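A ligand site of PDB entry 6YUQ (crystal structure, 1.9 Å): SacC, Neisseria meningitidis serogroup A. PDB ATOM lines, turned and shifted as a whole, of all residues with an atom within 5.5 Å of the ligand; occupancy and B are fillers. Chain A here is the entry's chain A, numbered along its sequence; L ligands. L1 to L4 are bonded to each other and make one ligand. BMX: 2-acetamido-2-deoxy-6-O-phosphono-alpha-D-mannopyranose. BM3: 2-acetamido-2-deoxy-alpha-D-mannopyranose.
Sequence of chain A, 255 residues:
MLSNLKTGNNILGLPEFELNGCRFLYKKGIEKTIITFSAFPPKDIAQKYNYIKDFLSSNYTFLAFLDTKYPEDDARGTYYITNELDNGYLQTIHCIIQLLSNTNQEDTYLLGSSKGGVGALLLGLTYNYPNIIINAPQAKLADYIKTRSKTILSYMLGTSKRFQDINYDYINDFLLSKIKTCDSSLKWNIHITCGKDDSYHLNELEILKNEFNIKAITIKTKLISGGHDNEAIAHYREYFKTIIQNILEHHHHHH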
ATOM      1  N   SER A  38     -15.073 -13.734   0.751  1.00  0.00           N
ATOM      2  CA  SER A  38     -16.033 -14.598   1.438  1.00  0.00           C
ATOM      3  C   SER A  38     -17.160 -13.771   2.041  1.00  0.00           C
ATOM      4  O   SER A  38     -16.972 -12.628   2.473  1.00  0.00           O
ATOM      5  CB  SER A  38     -15.329 -15.389   2.539  1.00  0.00           C
ATOM      6  OG  SER A  38     -16.243 -16.068   3.382  1.00  0.00           O
ATOM      7  N   ALA A  39     -18.350 -14.369   2.075  1.00  0.00           N
ATOM      8  CA  ALA A  39     -19.521 -13.783   2.720  1.00  0.00           C
ATOM      9  C   ALA A  39     -19.727 -14.381   4.113  1.00  0.00           C
ATOM     10  O   ALA A  39     -18.993 -15.277   4.542  1.00  0.00           O
ATOM     11  CB  ALA A  39     -20.764 -13.987   1.863  1.00  0.00           C
ATOM     12  N   PHE A  40     -20.718 -13.867   4.836  1.00  0.00           N
ATOM     13  CA  PHE A  40     -21.092 -14.412   6.152  1.00  0.00           C
ATOM     14  C   PHE A  40     -21.655 -15.813   5.976  1.00  0.00           C
ATOM     15  O   PHE A  40     -22.702 -15.967   5.331  1.00  0.00           O
ATOM     16  CB  PHE A  40     -22.162 -13.539   6.854  1.00  0.00           C
ATOM     17  CG  PHE A  40     -21.587 -12.452   7.728  1.00  0.00           C
ATOM     18  CD1 PHE A  40     -20.459 -12.680   8.496  1.00  0.00           C
ATOM     19  CD2 PHE A  40     -22.195 -11.207   7.790  1.00  0.00           C
ATOM     20  CE1 PHE A  40     -19.925 -11.679   9.303  1.00  0.00           C
ATOM     21  CE2 PHE A  40     -21.668 -10.194   8.594  1.00  0.00           C
ATOM     22  CZ  PHE A  40     -20.530 -10.436   9.352  1.00  0.00           C
ATOM     23  N   PRO A  41     -21.021 -16.854   6.496  1.00  0.00           N
ATOM     24  CA  PRO A  41     -21.618 -18.190   6.464  1.00  0.00           C
ATOM     25  C   PRO A  41     -22.656 -18.313   7.562  1.00  0.00           C
ATOM     26  O   PRO A  41     -22.733 -17.446   8.446  1.00  0.00           O
ATOM     27  CB  PRO A  41     -20.416 -19.099   6.728  1.00  0.00           C
ATOM     28  CG  PRO A  41     -19.567 -18.294   7.655  1.00  0.00           C
ATOM     29  CD  PRO A  41     -19.719 -16.850   7.189  1.00  0.00           C
ATOM     30  N   PRO A  42     -23.497 -19.358   7.537  1.00  0.00           N
ATOM     31  CA  PRO A  42     -24.422 -19.581   8.658  1.00  0.00           C
ATOM     32  C   PRO A  42     -23.650 -19.816   9.945  1.00  0.00           C
ATOM     33  O   PRO A  42     -22.474 -20.187   9.949  1.00  0.00           O
ATOM     34  CB  PRO A  42     -25.208 -20.837   8.243  1.00  0.00           C
ATOM     35  CG  PRO A  42     -25.053 -20.897   6.753  1.00  0.00           C
ATOM     36  CD  PRO A  42     -23.660 -20.380   6.490  1.00  0.00           C
ATOM     37  N   LYS A  43     -24.340 -19.617  11.068  1.00  0.00           N
ATOM     38  CA  LYS A  43     -23.695 -19.741  12.363  1.00  0.00           C
ATOM     39  C   LYS A  43     -23.157 -21.155  12.548  1.00  0.00           C
ATOM     40  O   LYS A  43     -23.772 -22.136  12.118  1.00  0.00           O
ATOM     41  CB  LYS A  43     -24.673 -19.397  13.496  1.00  0.00           C
ATOM     42  CG  LYS A  43     -24.086 -19.599  14.892  1.00  0.00           C
ATOM     43  CD  LYS A  43     -24.960 -18.999  15.984  1.00  0.00           C
ATOM     44  CE  LYS A  43     -24.614 -19.580  17.346  1.00  0.00           C
ATOM     45  NZ  LYS A  43     -23.291 -19.073  17.822  1.00  0.00           N
ATOM     46  N   LYS A  48     -16.079 -19.656   4.031  1.00  0.00           N
ATOM     47  CA  LYS A  48     -15.886 -20.414   2.803  1.00  0.00           C
ATOM     48  C   LYS A  48     -15.246 -19.544   1.719  1.00  0.00           C
ATOM     49  O   LYS A  48     -15.593 -18.367   1.576  1.00  0.00           O
ATOM     50  CB  LYS A  48     -17.210 -20.989   2.301  1.00  0.00           C
ATOM     51  N   TYR A  49     -14.314 -20.129   0.975  1.00  0.00           N
ATOM     52  CA  TYR A  49     -13.786 -19.475  -0.205  1.00  0.00           C
ATOM     53  C   TYR A  49     -14.811 -19.531  -1.327  1.00  0.00           C
ATOM     54  O   TYR A  49     -15.530 -20.519  -1.474  1.00  0.00           O
ATOM     55  CB  TYR A  49     -12.475 -20.133  -0.643  1.00  0.00           C
ATOM     56  CG  TYR A  49     -11.370 -19.990   0.368  1.00  0.00           C
ATOM     57  CD1 TYR A  49     -10.623 -18.827   0.448  1.00  0.00           C
ATOM     58  CD2 TYR A  49     -11.063 -21.029   1.250  1.00  0.00           C
ATOM     59  CE1 TYR A  49      -9.609 -18.678   1.370  1.00  0.00           C
ATOM     60  CE2 TYR A  49     -10.030 -20.895   2.172  1.00  0.00           C
ATOM     61  CZ  TYR A  49      -9.313 -19.712   2.232  1.00  0.00           C
ATOM     62  OH  TYR A  49      -8.292 -19.549   3.138  1.00  0.00           O
ATOM     63  N   ASN A  50     -14.891 -18.473  -2.109  1.00  0.00           N
ATOM     64  CA  ASN A  50     -15.980 -18.286  -3.053  1.00  0.00           C
ATOM     65  C   ASN A  50     -15.518 -18.503  -4.493  1.00  0.00           C
ATOM     66  O   ASN A  50     -14.439 -18.046  -4.892  1.00  0.00           O
ATOM     67  CB  ASN A  50     -16.577 -16.891  -2.908  1.00  0.00           C
ATOM     68  CG  ASN A  50     -17.709 -16.839  -1.909  1.00  0.00           C
ATOM     69  OD1 ASN A  50     -17.544 -17.167  -0.730  1.00  0.00           O
ATOM     70  ND2 ASN A  50     -18.872 -16.443  -2.371  1.00  0.00           N
ATOM     71  N   TYR A  51     -16.354 -19.211  -5.253  1.00  0.00           N
ATOM     72  CA  TYR A  51     -16.261 -19.336  -6.714  1.00  0.00           C
ATOM     73  C   TYR A  51     -15.003 -20.078  -7.169  1.00  0.00           C
ATOM     74  O   TYR A  51     -14.518 -19.836  -8.275  1.00  0.00           O
ATOM     75  CB  TYR A  51     -16.358 -17.968  -7.390  1.00  0.00           C
ATOM     76  CG  TYR A  51     -17.437 -17.087  -6.774  1.00  0.00           C
ATOM     77  CD1 TYR A  51     -18.705 -17.587  -6.481  1.00  0.00           C
ATOM     78  CD2 TYR A  51     -17.170 -15.768  -6.483  1.00  0.00           C
ATOM     79  CE1 TYR A  51     -19.681 -16.789  -5.901  1.00  0.00           C
ATOM     80  CE2 TYR A  51     -18.121 -14.950  -5.906  1.00  0.00           C
ATOM     81  CZ  TYR A  51     -19.370 -15.459  -5.621  1.00  0.00           C
ATOM     82  OH  TYR A  51     -20.293 -14.609  -5.040  1.00  0.00           O
ATOM     83  N   LYS A  53     -14.867 -23.266  -8.042  1.00  0.00           N
ATOM     84  CA  LYS A  53     -15.168 -24.146  -9.166  1.00  0.00           C
ATOM     85  C   LYS A  53     -15.371 -23.388 -10.469  1.00  0.00           C
ATOM     86  O   LYS A  53     -15.232 -23.990 -11.546  1.00  0.00           O
ATOM     87  CB  LYS A  53     -16.398 -24.999  -8.844  1.00  0.00           C
ATOM     88  CG  LYS A  53     -16.389 -25.620  -7.454  1.00  0.00           C
ATOM     89  CD  LYS A  53     -17.564 -26.571  -7.286  1.00  0.00           C
ATOM     90  CE  LYS A  53     -17.761 -26.968  -5.827  1.00  0.00           C
ATOM     91  NZ  LYS A  53     -19.129 -27.506  -5.567  1.00  0.00           N
ATOM     92  N   ARG A  76     -16.843 -15.548  12.211  1.00  0.00           N
ATOM     93  CA  ARG A  76     -17.272 -15.377  10.825  1.00  0.00           C
ATOM     94  C   ARG A  76     -16.817 -14.067  10.214  1.00  0.00           C
ATOM     95  O   ARG A  76     -17.222 -13.752   9.090  1.00  0.00           O
ATOM     96  CB  ARG A  76     -18.798 -15.505  10.745  1.00  0.00           C
ATOM     97  CG  ARG A  76     -19.254 -16.926  11.006  1.00  0.00           C
ATOM     98  CD  ARG A  76     -20.770 -17.058  10.945  1.00  0.00           C
ATOM     99  NE  ARG A  76     -21.438 -16.547  12.148  1.00  0.00           N
ATOM    100  CZ  ARG A  76     -22.734 -16.249  12.187  1.00  0.00           C
ATOM    101  NH1 ARG A  76     -23.494 -16.414  11.123  1.00  0.00           N
ATOM    102  NH2 ARG A  76     -23.273 -15.809  13.322  1.00  0.00           N
ATOM    103  N   SER A 113     -20.319 -11.612  -3.112  1.00  0.00           N
ATOM    104  CA  SER A 113     -21.748 -11.387  -2.915  1.00  0.00           C
ATOM    105  C   SER A 113     -22.005 -11.065  -1.451  1.00  0.00           C
ATOM    106  O   SER A 113     -21.336 -11.621  -0.561  1.00  0.00           O
ATOM    107  CB  SER A 113     -22.566 -12.615  -3.367  1.00  0.00           C
ATOM    108  OG  SER A 113     -23.949 -12.438  -3.086  1.00  0.00           O
ATOM    109  N   SER A 114     -22.950 -10.161  -1.195  1.00  0.00           N
ATOM    110  CA  SER A 114     -23.338  -9.763   0.177  1.00  0.00           C
ATOM    111  C   SER A 114     -22.113  -9.195   0.882  1.00  0.00           C
ATOM    112  O   SER A 114     -21.548  -8.209   0.378  1.00  0.00           O
ATOM    113  CB  SER A 114     -24.000 -10.953   0.866  1.00  0.00           C
ATOM    114  OG  SER A 114     -24.730 -10.535   2.012  1.00  0.00           O
ATOM    115  N   LYS A 115     -21.695  -9.738   2.027  1.00  0.00           N
ATOM    116  CA  LYS A 115     -20.505  -9.221   2.708  1.00  0.00           C
ATOM    117  C   LYS A 115     -19.281  -9.321   1.798  1.00  0.00           C
ATOM    118  O   LYS A 115     -18.391  -8.467   1.850  1.00  0.00           O
ATOM    119  CB  LYS A 115     -20.257  -9.973   4.009  1.00  0.00           C
ATOM    120  CG  LYS A 115     -19.059  -9.435   4.816  1.00  0.00           C
ATOM    121  CD  LYS A 115     -18.717 -10.326   6.006  1.00  0.00           C
ATOM    122  CE  LYS A 115     -17.965 -11.580   5.577  1.00  0.00           C
ATOM    123  NZ  LYS A 115     -17.420 -12.343   6.734  1.00  0.00           N
ATOM    124  N   ASN A 135     -22.547  -8.860  -6.154  1.00  0.00           N
ATOM    125  CA  ASN A 135     -23.981  -9.064  -6.011  1.00  0.00           C
ATOM    126  C   ASN A 135     -24.433  -8.626  -4.622  1.00  0.00           C
ATOM    127  O   ASN A 135     -23.739  -8.879  -3.634  1.00  0.00           O
ATOM    128  CB  ASN A 135     -24.368 -10.524  -6.240  1.00  0.00           C
ATOM    129  CG  ASN A 135     -25.853 -10.766  -6.032  1.00  0.00           C
ATOM    130  OD1 ASN A 135     -26.673 -10.343  -6.841  1.00  0.00           O
ATOM    131  ND2 ASN A 135     -26.194 -11.427  -4.934  1.00  0.00           N
ATOM    132  N   TYR A 144     -26.882  -4.346   9.107  1.00  0.00           N
ATOM    133  CA  TYR A 144     -26.951  -5.702   8.600  1.00  0.00           C
ATOM    134  C   TYR A 144     -26.304  -6.701   9.546  1.00  0.00           C
ATOM    135  O   TYR A 144     -26.822  -7.807   9.724  1.00  0.00           O
ATOM    136  CB  TYR A 144     -26.313  -5.799   7.218  1.00  0.00           C
ATOM    137  CG  TYR A 144     -26.435  -7.195   6.626  1.00  0.00           C
ATOM    138  CD1 TYR A 144     -27.653  -7.649   6.122  1.00  0.00           C
ATOM    139  CD2 TYR A 144     -25.347  -8.055   6.574  1.00  0.00           C
ATOM    140  CE1 TYR A 144     -27.789  -8.920   5.578  1.00  0.00           C
ATOM    141  CE2 TYR A 144     -25.468  -9.333   6.036  1.00  0.00           C
ATOM    142  CZ  TYR A 144     -26.689  -9.763   5.534  1.00  0.00           C
ATOM    143  OH  TYR A 144     -26.822 -11.021   4.997  1.00  0.00           O
ATOM    144  N   LYS A 146     -26.240  -6.501  12.653  1.00  0.00           N
ATOM    145  CA  LYS A 146     -27.219  -6.671  13.718  1.00  0.00           C
ATOM    146  C   LYS A 146     -28.190  -7.791  13.401  1.00  0.00           C
ATOM    147  O   LYS A 146     -28.596  -8.547  14.292  1.00  0.00           O
ATOM    148  CB  LYS A 146     -27.974  -5.357  13.940  1.00  0.00           C
ATOM    149  CG  LYS A 146     -28.735  -5.279  15.233  1.00  0.00           C
ATOM    150  CD  LYS A 146     -29.159  -3.851  15.526  1.00  0.00           C
ATOM    151  CE  LYS A 146     -30.288  -3.412  14.623  1.00  0.00           C
ATOM    152  NZ  LYS A 146     -31.248  -2.563  15.380  1.00  0.00           N
ATOM    153  N   THR A 147     -28.570  -7.927  12.137  1.00  0.00           N
ATOM    154  CA  THR A 147     -29.525  -8.960  11.728  1.00  0.00           C
ATOM    155  C   THR A 147     -28.886 -10.318  11.507  1.00  0.00           C
ATOM    156  O   THR A 147     -29.599 -11.273  11.183  1.00  0.00           O
ATOM    157  CB  THR A 147     -30.247  -8.550  10.441  1.00  0.00           C
ATOM    158  OG1 THR A 147     -29.402  -8.833   9.322  1.00  0.00           O
ATOM    159  CG2 THR A 147     -30.586  -7.064  10.457  1.00  0.00           C
ATOM    160  N   ARG A 148     -27.568 -10.447  11.664  1.00  0.00           N
ATOM    161  CA  ARG A 148     -26.864 -11.697  11.392  1.00  0.00           C
ATOM    162  C   ARG A 148     -26.192 -12.297  12.614  1.00  0.00           C
ATOM    163  O   ARG A 148     -26.186 -13.523  12.770  1.00  0.00           O
ATOM    164  CB  ARG A 148     -25.805 -11.488  10.293  1.00  0.00           C
ATOM    165  CG  ARG A 148     -26.381 -11.346   8.896  1.00  0.00           C
ATOM    166  CD  ARG A 148     -27.272 -12.541   8.528  1.00  0.00           C
ATOM    167  NE  ARG A 148     -26.515 -13.798   8.522  1.00  0.00           N
ATOM    168  CZ  ARG A 148     -25.735 -14.170   7.512  1.00  0.00           C
ATOM    169  NH1 ARG A 148     -25.616 -13.387   6.450  1.00  0.00           N
ATOM    170  NH2 ARG A 148     -25.071 -15.317   7.578  1.00  0.00           N
ATOM    171  N   SER A 149     -25.605 -11.475  13.500  1.00  0.00           N
ATOM    172  CA  SER A 149     -24.954 -11.994  14.700  1.00  0.00           C
ATOM    173  C   SER A 149     -24.784 -10.840  15.681  1.00  0.00           C
ATOM    174  O   SER A 149     -24.013  -9.908  15.410  1.00  0.00           O
ATOM    175  CB  SER A 149     -23.601 -12.620  14.368  1.00  0.00           C
ATOM    176  OG  SER A 149     -22.750 -12.611  15.495  1.00  0.00           O
ATOM    177  N   LYS A 150     -25.473 -10.928  16.816  1.00  0.00           N
ATOM    178  CA  LYS A 150     -25.256  -9.940  17.872  1.00  0.00           C
ATOM    179  C   LYS A 150     -23.861 -10.056  18.464  1.00  0.00           C
ATOM    180  O   LYS A 150     -23.284  -9.056  18.909  1.00  0.00           O
ATOM    181  CB  LYS A 150     -26.322 -10.091  18.958  1.00  0.00           C
ATOM    182  CG  LYS A 150     -27.740  -9.794  18.469  1.00  0.00           C
ATOM    183  CD  LYS A 150     -27.968  -8.304  18.233  1.00  0.00           C
ATOM    184  CE  LYS A 150     -29.442  -7.960  18.042  1.00  0.00           C
ATOM    185  NZ  LYS A 150     -30.012  -8.517  16.784  1.00  0.00           N
ATOM    186  N   GLY A 227     -33.932 -14.033  -4.589  1.00  0.00           N
ATOM    187  CA  GLY A 227     -33.788 -13.127  -3.467  1.00  0.00           C
ATOM    188  C   GLY A 227     -32.342 -13.030  -3.038  1.00  0.00           C
ATOM    189  O   GLY A 227     -31.448 -12.968  -3.901  1.00  0.00           O
ATOM    190  N   HIS A 228     -32.099 -12.999  -1.725  1.00  0.00           N
ATOM    191  CA  HIS A 228     -30.757 -13.098  -1.152  1.00  0.00           C
ATOM    192  C   HIS A 228     -30.447 -14.568  -0.857  1.00  0.00           C
ATOM    193  O   HIS A 228     -30.304 -14.987   0.285  1.00  0.00           O
ATOM    194  CB  HIS A 228     -30.658 -12.249   0.115  1.00  0.00           C
ATOM    195  CG  HIS A 228     -29.287 -11.746   0.434  1.00  0.00           C
ATOM    196  ND1 HIS A 228     -28.758 -10.612  -0.145  1.00  0.00           N
ATOM    197  CD2 HIS A 228     -28.336 -12.222   1.279  1.00  0.00           C
ATOM    198  CE1 HIS A 228     -27.535 -10.415   0.330  1.00  0.00           C
ATOM    199  NE2 HIS A 228     -27.263 -11.370   1.194  1.00  0.00           N
ATOM    200  N   ASP A 229     -30.314 -15.340  -1.936  1.00  0.00           N
ATOM    201  CA  ASP A 229     -30.288 -16.802  -1.822  1.00  0.00           C
ATOM    202  C   ASP A 229     -29.382 -17.377  -2.915  1.00  0.00           C
ATOM    203  O   ASP A 229     -28.713 -16.646  -3.643  1.00  0.00           O
ATOM    204  CB  ASP A 229     -31.715 -17.365  -1.938  1.00  0.00           C
ATOM    205  CG  ASP A 229     -32.442 -16.828  -3.166  1.00  0.00           C
ATOM    206  OD1 ASP A 229     -31.796 -16.659  -4.216  1.00  0.00           O
ATOM    207  OD2 ASP A 229     -33.659 -16.563  -3.074  1.00  0.00           O
ATOM    208  N   ASN A 230     -29.406 -18.707  -3.044  1.00  0.00           N
ATOM    209  CA  ASN A 230     -28.565 -19.398  -4.010  1.00  0.00           C
ATOM    210  C   ASN A 230     -29.010 -19.198  -5.458  1.00  0.00           C
ATOM    211  O   ASN A 230     -28.188 -19.338  -6.367  1.00  0.00           O
ATOM    212  CB  ASN A 230     -28.538 -20.902  -3.678  1.00  0.00           C
ATOM    213  CG  ASN A 230     -27.510 -21.234  -2.600  1.00  0.00           C
ATOM    214  OD1 ASN A 230     -27.015 -20.352  -1.889  1.00  0.00           O
ATOM    215  ND2 ASN A 230     -27.173 -22.520  -2.494  1.00  0.00           N
ATOM    216  N   ILE A 233     -27.324 -16.040  -6.549  1.00  0.00           N
ATOM    217  CA  ILE A 233     -25.897 -16.340  -6.696  1.00  0.00           C
ATOM    218  C   ILE A 233     -25.643 -17.075  -7.999  1.00  0.00           C
ATOM    219  O   ILE A 233     -24.662 -16.798  -8.705  1.00  0.00           O
ATOM    220  CB  ILE A 233     -25.387 -17.126  -5.478  1.00  0.00           C
ATOM    221  CG1 ILE A 233     -25.171 -16.190  -4.279  1.00  0.00           C
ATOM    222  CG2 ILE A 233     -24.074 -17.828  -5.802  1.00  0.00           C
ATOM    223  CD1 ILE A 233     -25.021 -16.917  -2.976  1.00  0.00           C
ATOM    224  N   ARG A 237     -23.206 -15.673 -10.823  1.00  0.00           N
ATOM    225  CA  ARG A 237     -22.092 -16.425 -11.405  1.00  0.00           C
ATOM    226  C   ARG A 237     -22.132 -16.382 -12.930  1.00  0.00           C
ATOM    227  O   ARG A 237     -21.111 -16.192 -13.586  1.00  0.00           O
ATOM    228  CB  ARG A 237     -22.127 -17.882 -10.913  1.00  0.00           C
ATOM    229  CG  ARG A 237     -21.525 -18.128  -9.520  1.00  0.00           C
ATOM    230  CD  ARG A 237     -21.626 -19.591  -9.093  1.00  0.00           C
ATOM    231  NE  ARG A 237     -20.402 -20.375  -9.326  1.00  0.00           N
ATOM    232  CZ  ARG A 237     -19.916 -21.270  -8.465  1.00  0.00           C
ATOM    233  NH1 ARG A 237     -18.814 -21.933  -8.743  1.00  0.00           N
ATOM    234  NH2 ARG A 237     -20.522 -21.465  -7.308  1.00  0.00           N
HETATM  235  C1  BMX L   1     -20.733 -22.077  -2.009  1.00  0.00           C
HETATM  236  C2  BMX L   1     -21.877 -22.561  -2.883  1.00  0.00           C
HETATM  237  C3  BMX L   1     -23.172 -21.863  -2.575  1.00  0.00           C
HETATM  238  C4  BMX L   1     -23.020 -20.714  -1.607  1.00  0.00           C
HETATM  239  C5  BMX L   1     -21.807 -19.834  -1.923  1.00  0.00           C
HETATM  240  C6  BMX L   1     -21.552 -18.863  -0.778  1.00  0.00           C
HETATM  241  C7  BMX L   1     -21.719 -24.957  -3.836  1.00  0.00           C
HETATM  242  C8  BMX L   1     -21.240 -24.374  -5.200  1.00  0.00           C
HETATM  243  N2  BMX L   1     -22.026 -24.051  -2.708  1.00  0.00           N
HETATM  244  O1  BMX L   1     -19.578 -22.748  -2.344  1.00  0.00           O
HETATM  245  O3  BMX L   1     -24.128 -22.818  -2.043  1.00  0.00           O
HETATM  246  O4  BMX L   1     -24.220 -19.919  -1.624  1.00  0.00           O
HETATM  247  O5  BMX L   1     -20.560 -20.594  -2.168  1.00  0.00           O
HETATM  248  O6  BMX L   1     -22.270 -19.313   0.389  1.00  0.00           O
HETATM  249  O7  BMX L   1     -21.825 -26.124  -3.703  1.00  0.00           O
HETATM  250  P   BMX L   1     -21.951 -18.579   1.889  1.00  0.00           P
HETATM  251  O19 BMX L   1     -20.463 -18.377   2.050  1.00  0.00           O
HETATM  252  O17 BMX L   1     -22.442 -19.476   3.011  1.00  0.00           O
HETATM  253  O18 BMX L   1     -22.715 -17.109   1.945  1.00  0.00           O
HETATM  254  C1  BMX L   2     -23.894 -16.936   1.291  1.00  0.00           C
HETATM  255  C2  BMX L   2     -24.302 -15.474   1.417  1.00  0.00           C
HETATM  256  C3  BMX L   2     -24.655 -15.102   2.805  1.00  0.00           C
HETATM  257  C4  BMX L   2     -25.681 -16.054   3.382  1.00  0.00           C
HETATM  258  C5  BMX L   2     -25.161 -17.502   3.297  1.00  0.00           C
HETATM  259  C6  BMX L   2     -26.133 -18.475   3.902  1.00  0.00           C
HETATM  260  C7  BMX L   2     -25.436 -14.347  -0.585  1.00  0.00           C
HETATM  261  C8  BMX L   2     -26.694 -14.076  -1.417  1.00  0.00           C
HETATM  262  N2  BMX L   2     -25.523 -15.207   0.590  1.00  0.00           N
HETATM  263  O3  BMX L   2     -25.164 -13.744   2.804  1.00  0.00           O
HETATM  264  O4  BMX L   2     -25.955 -15.722   4.726  1.00  0.00           O
HETATM  265  O5  BMX L   2     -24.913 -17.869   1.890  1.00  0.00           O
HETATM  266  O6  BMX L   2     -27.453 -18.176   3.391  1.00  0.00           O
HETATM  267  O7  BMX L   2     -24.385 -13.856  -0.893  1.00  0.00           O
HETATM  268  P   BMX L   2     -28.493 -19.452   3.110  1.00  0.00           P
HETATM  269  O19 BMX L   2     -27.686 -20.732   2.936  1.00  0.00           O
HETATM  270  O17 BMX L   2     -29.335 -19.177   1.876  1.00  0.00           O
HETATM  271  O18 BMX L   2     -29.496 -19.624   4.453  1.00  0.00           O
HETATM  272  C1  BMX L   3     -28.958 -20.239   5.567  1.00  0.00           C
HETATM  273  C2  BMX L   3     -30.073 -20.783   6.428  1.00  0.00           C
HETATM  274  C3  BMX L   3     -30.963 -19.706   6.889  1.00  0.00           C
HETATM  275  C4  BMX L   3     -30.203 -18.609   7.586  1.00  0.00           C
HETATM  276  C5  BMX L   3     -29.002 -18.109   6.783  1.00  0.00           C
HETATM  277  C6  BMX L   3     -28.167 -17.212   7.682  1.00  0.00           C
HETATM  278  C7  BMX L   3     -29.430 -22.915   7.765  1.00  0.00           C
HETATM  279  C8  BMX L   3     -30.081 -23.801   6.690  1.00  0.00           C
HETATM  280  N2  BMX L   3     -29.438 -21.457   7.636  1.00  0.00           N
HETATM  281  O3  BMX L   3     -31.969 -20.253   7.793  1.00  0.00           O
HETATM  282  O4  BMX L   3     -31.105 -17.513   7.830  1.00  0.00           O
HETATM  283  O5  BMX L   3     -28.150 -19.213   6.300  1.00  0.00           O
HETATM  284  O6  BMX L   3     -27.768 -18.009   8.792  1.00  0.00           O
HETATM  285  O7  BMX L   3     -28.919 -23.406   8.721  1.00  0.00           O
HETATM  286  P   BMX L   3     -27.314 -17.234  10.207  1.00  0.00           P
HETATM  287  O19 BMX L   3     -25.890 -16.775  10.069  1.00  0.00           O
HETATM  288  O17 BMX L   3     -27.384 -18.101  11.435  1.00  0.00           O
HETATM  289  O18 BMX L   3     -28.214 -15.815  10.320  1.00  0.00           O
HETATM  290  C1  BM3 L   4     -29.386 -15.727  11.022  1.00  0.00           C
HETATM  291  C2  BM3 L   4     -30.223 -14.621  10.389  1.00  0.00           C
HETATM  292  N2  BM3 L   4     -30.509 -14.862   8.918  1.00  0.00           N
HETATM  293  C7  BM3 L   4     -30.790 -13.708   8.040  1.00  0.00           C
HETATM  294  O7  BM3 L   4     -30.808 -12.606   8.496  1.00  0.00           O
HETATM  295  C8  BM3 L   4     -31.071 -13.934   6.508  1.00  0.00           C
HETATM  296  C3  BM3 L   4     -31.485 -14.447  11.160  1.00  0.00           C
HETATM  297  O3  BM3 L   4     -32.269 -15.675  11.095  1.00  0.00           O
HETATM  298  C4  BM3 L   4     -31.189 -14.153  12.602  1.00  0.00           C
HETATM  299  O4  BM3 L   4     -31.754 -12.861  12.881  1.00  0.00           O
HETATM  300  C5  BM3 L   4     -29.670 -14.149  12.890  1.00  0.00           C
HETATM  301  C6  BM3 L   4     -29.373 -13.954  14.380  1.00  0.00           C
HETATM  302  O6  BM3 L   4     -29.095 -12.579  14.574  1.00  0.00           O
HETATM  303  O5  BM3 L   4     -29.029 -15.390  12.446  1.00  0.00           O
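Merely in contact with the ligand: Ile 233 (3.4 Å), Pro 42 (3.5 Å), His 228 (3.6 Å), Lys 53 (3.6 Å), Pro 41 (3.6 Å), Arg 237 (3.7 Å), Ala 39 (3.7 Å), Ser 149 (3.8 Å), Asp 229 (3.9 Å), Tyr 144 (3.9 Å) and Asn 50 (3.9 Å). Hydrophobic or aromatic side chains within 4 Å of the ligand: Ala 39, Pro 42, His 228 and Ile 233.
NH1 of Arg 76 is in salt-bridge range of O19 of BMX L3 (2.6 Å). The side-chain hydroxyl of Ser 113 is in hydrogen-bond range of an oxygen (O7) of BMX L2, 2.6 Å away. The side-chain amide oxygen (OD1) of Asn 230 lies within hydrogen-bond range of an oxygen (O4) of BMX L1 (2.8 Å). The guanidinium group (NH2) of Arg 148 is in salt-bridge range of an oxygen (O19) of BMX L3, 3.0 Å away. O of Thr 147 lies within hydrogen-bond range of O4 of BM3 L4 (3.2 Å). O4 of BMX L2 lies close to O of Phe 40 (3.3 Å). OG of Ser 114 sits at hydrogen-bond distance from O3 of BMX L2, 3.3 Å away. The backbone NH (N) of Lys 43 sits at hydrogen-bond distance from an oxygen (O19) of BMX L3, at 3.4 Å.
The backbone carbonyl oxygen (O) of Arg 76 sits at hydrogen-bond distance from the side-chain amino group (NZ) of Lys 115 (2.8 Å). The side-chain hydroxyl (OG) of Ser 113 sits at hydrogen-bond distance from the side-chain amide nitrogen (ND2) of Asn 135. The guanidinium group of Arg 148 is in hydrogen-bond range of the backbone carbonyl oxygen of Phe 40 (3.3 Å). OH of Tyr 144 lies within hydrogen-bond range of NH1 of Arg 148, 3.0 Å away. The backbone carbonyl oxygen (O) of Tyr 144 lies within hydrogen-bond range of the side-chain hydroxyl (OG1) of Thr 147 (2.8 Å). N of Ser 114 lies within hydrogen-bond range of O of Asn 135 (2.9 Å). The side-chain carboxylate (OD2) of Asp 229 is in hydrogen-bond range of the backbone NH (N) of Gly 227, 3.0 Å away. OD1 of Asn 50 lies close to O of Lys 48 (3.3 Å).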
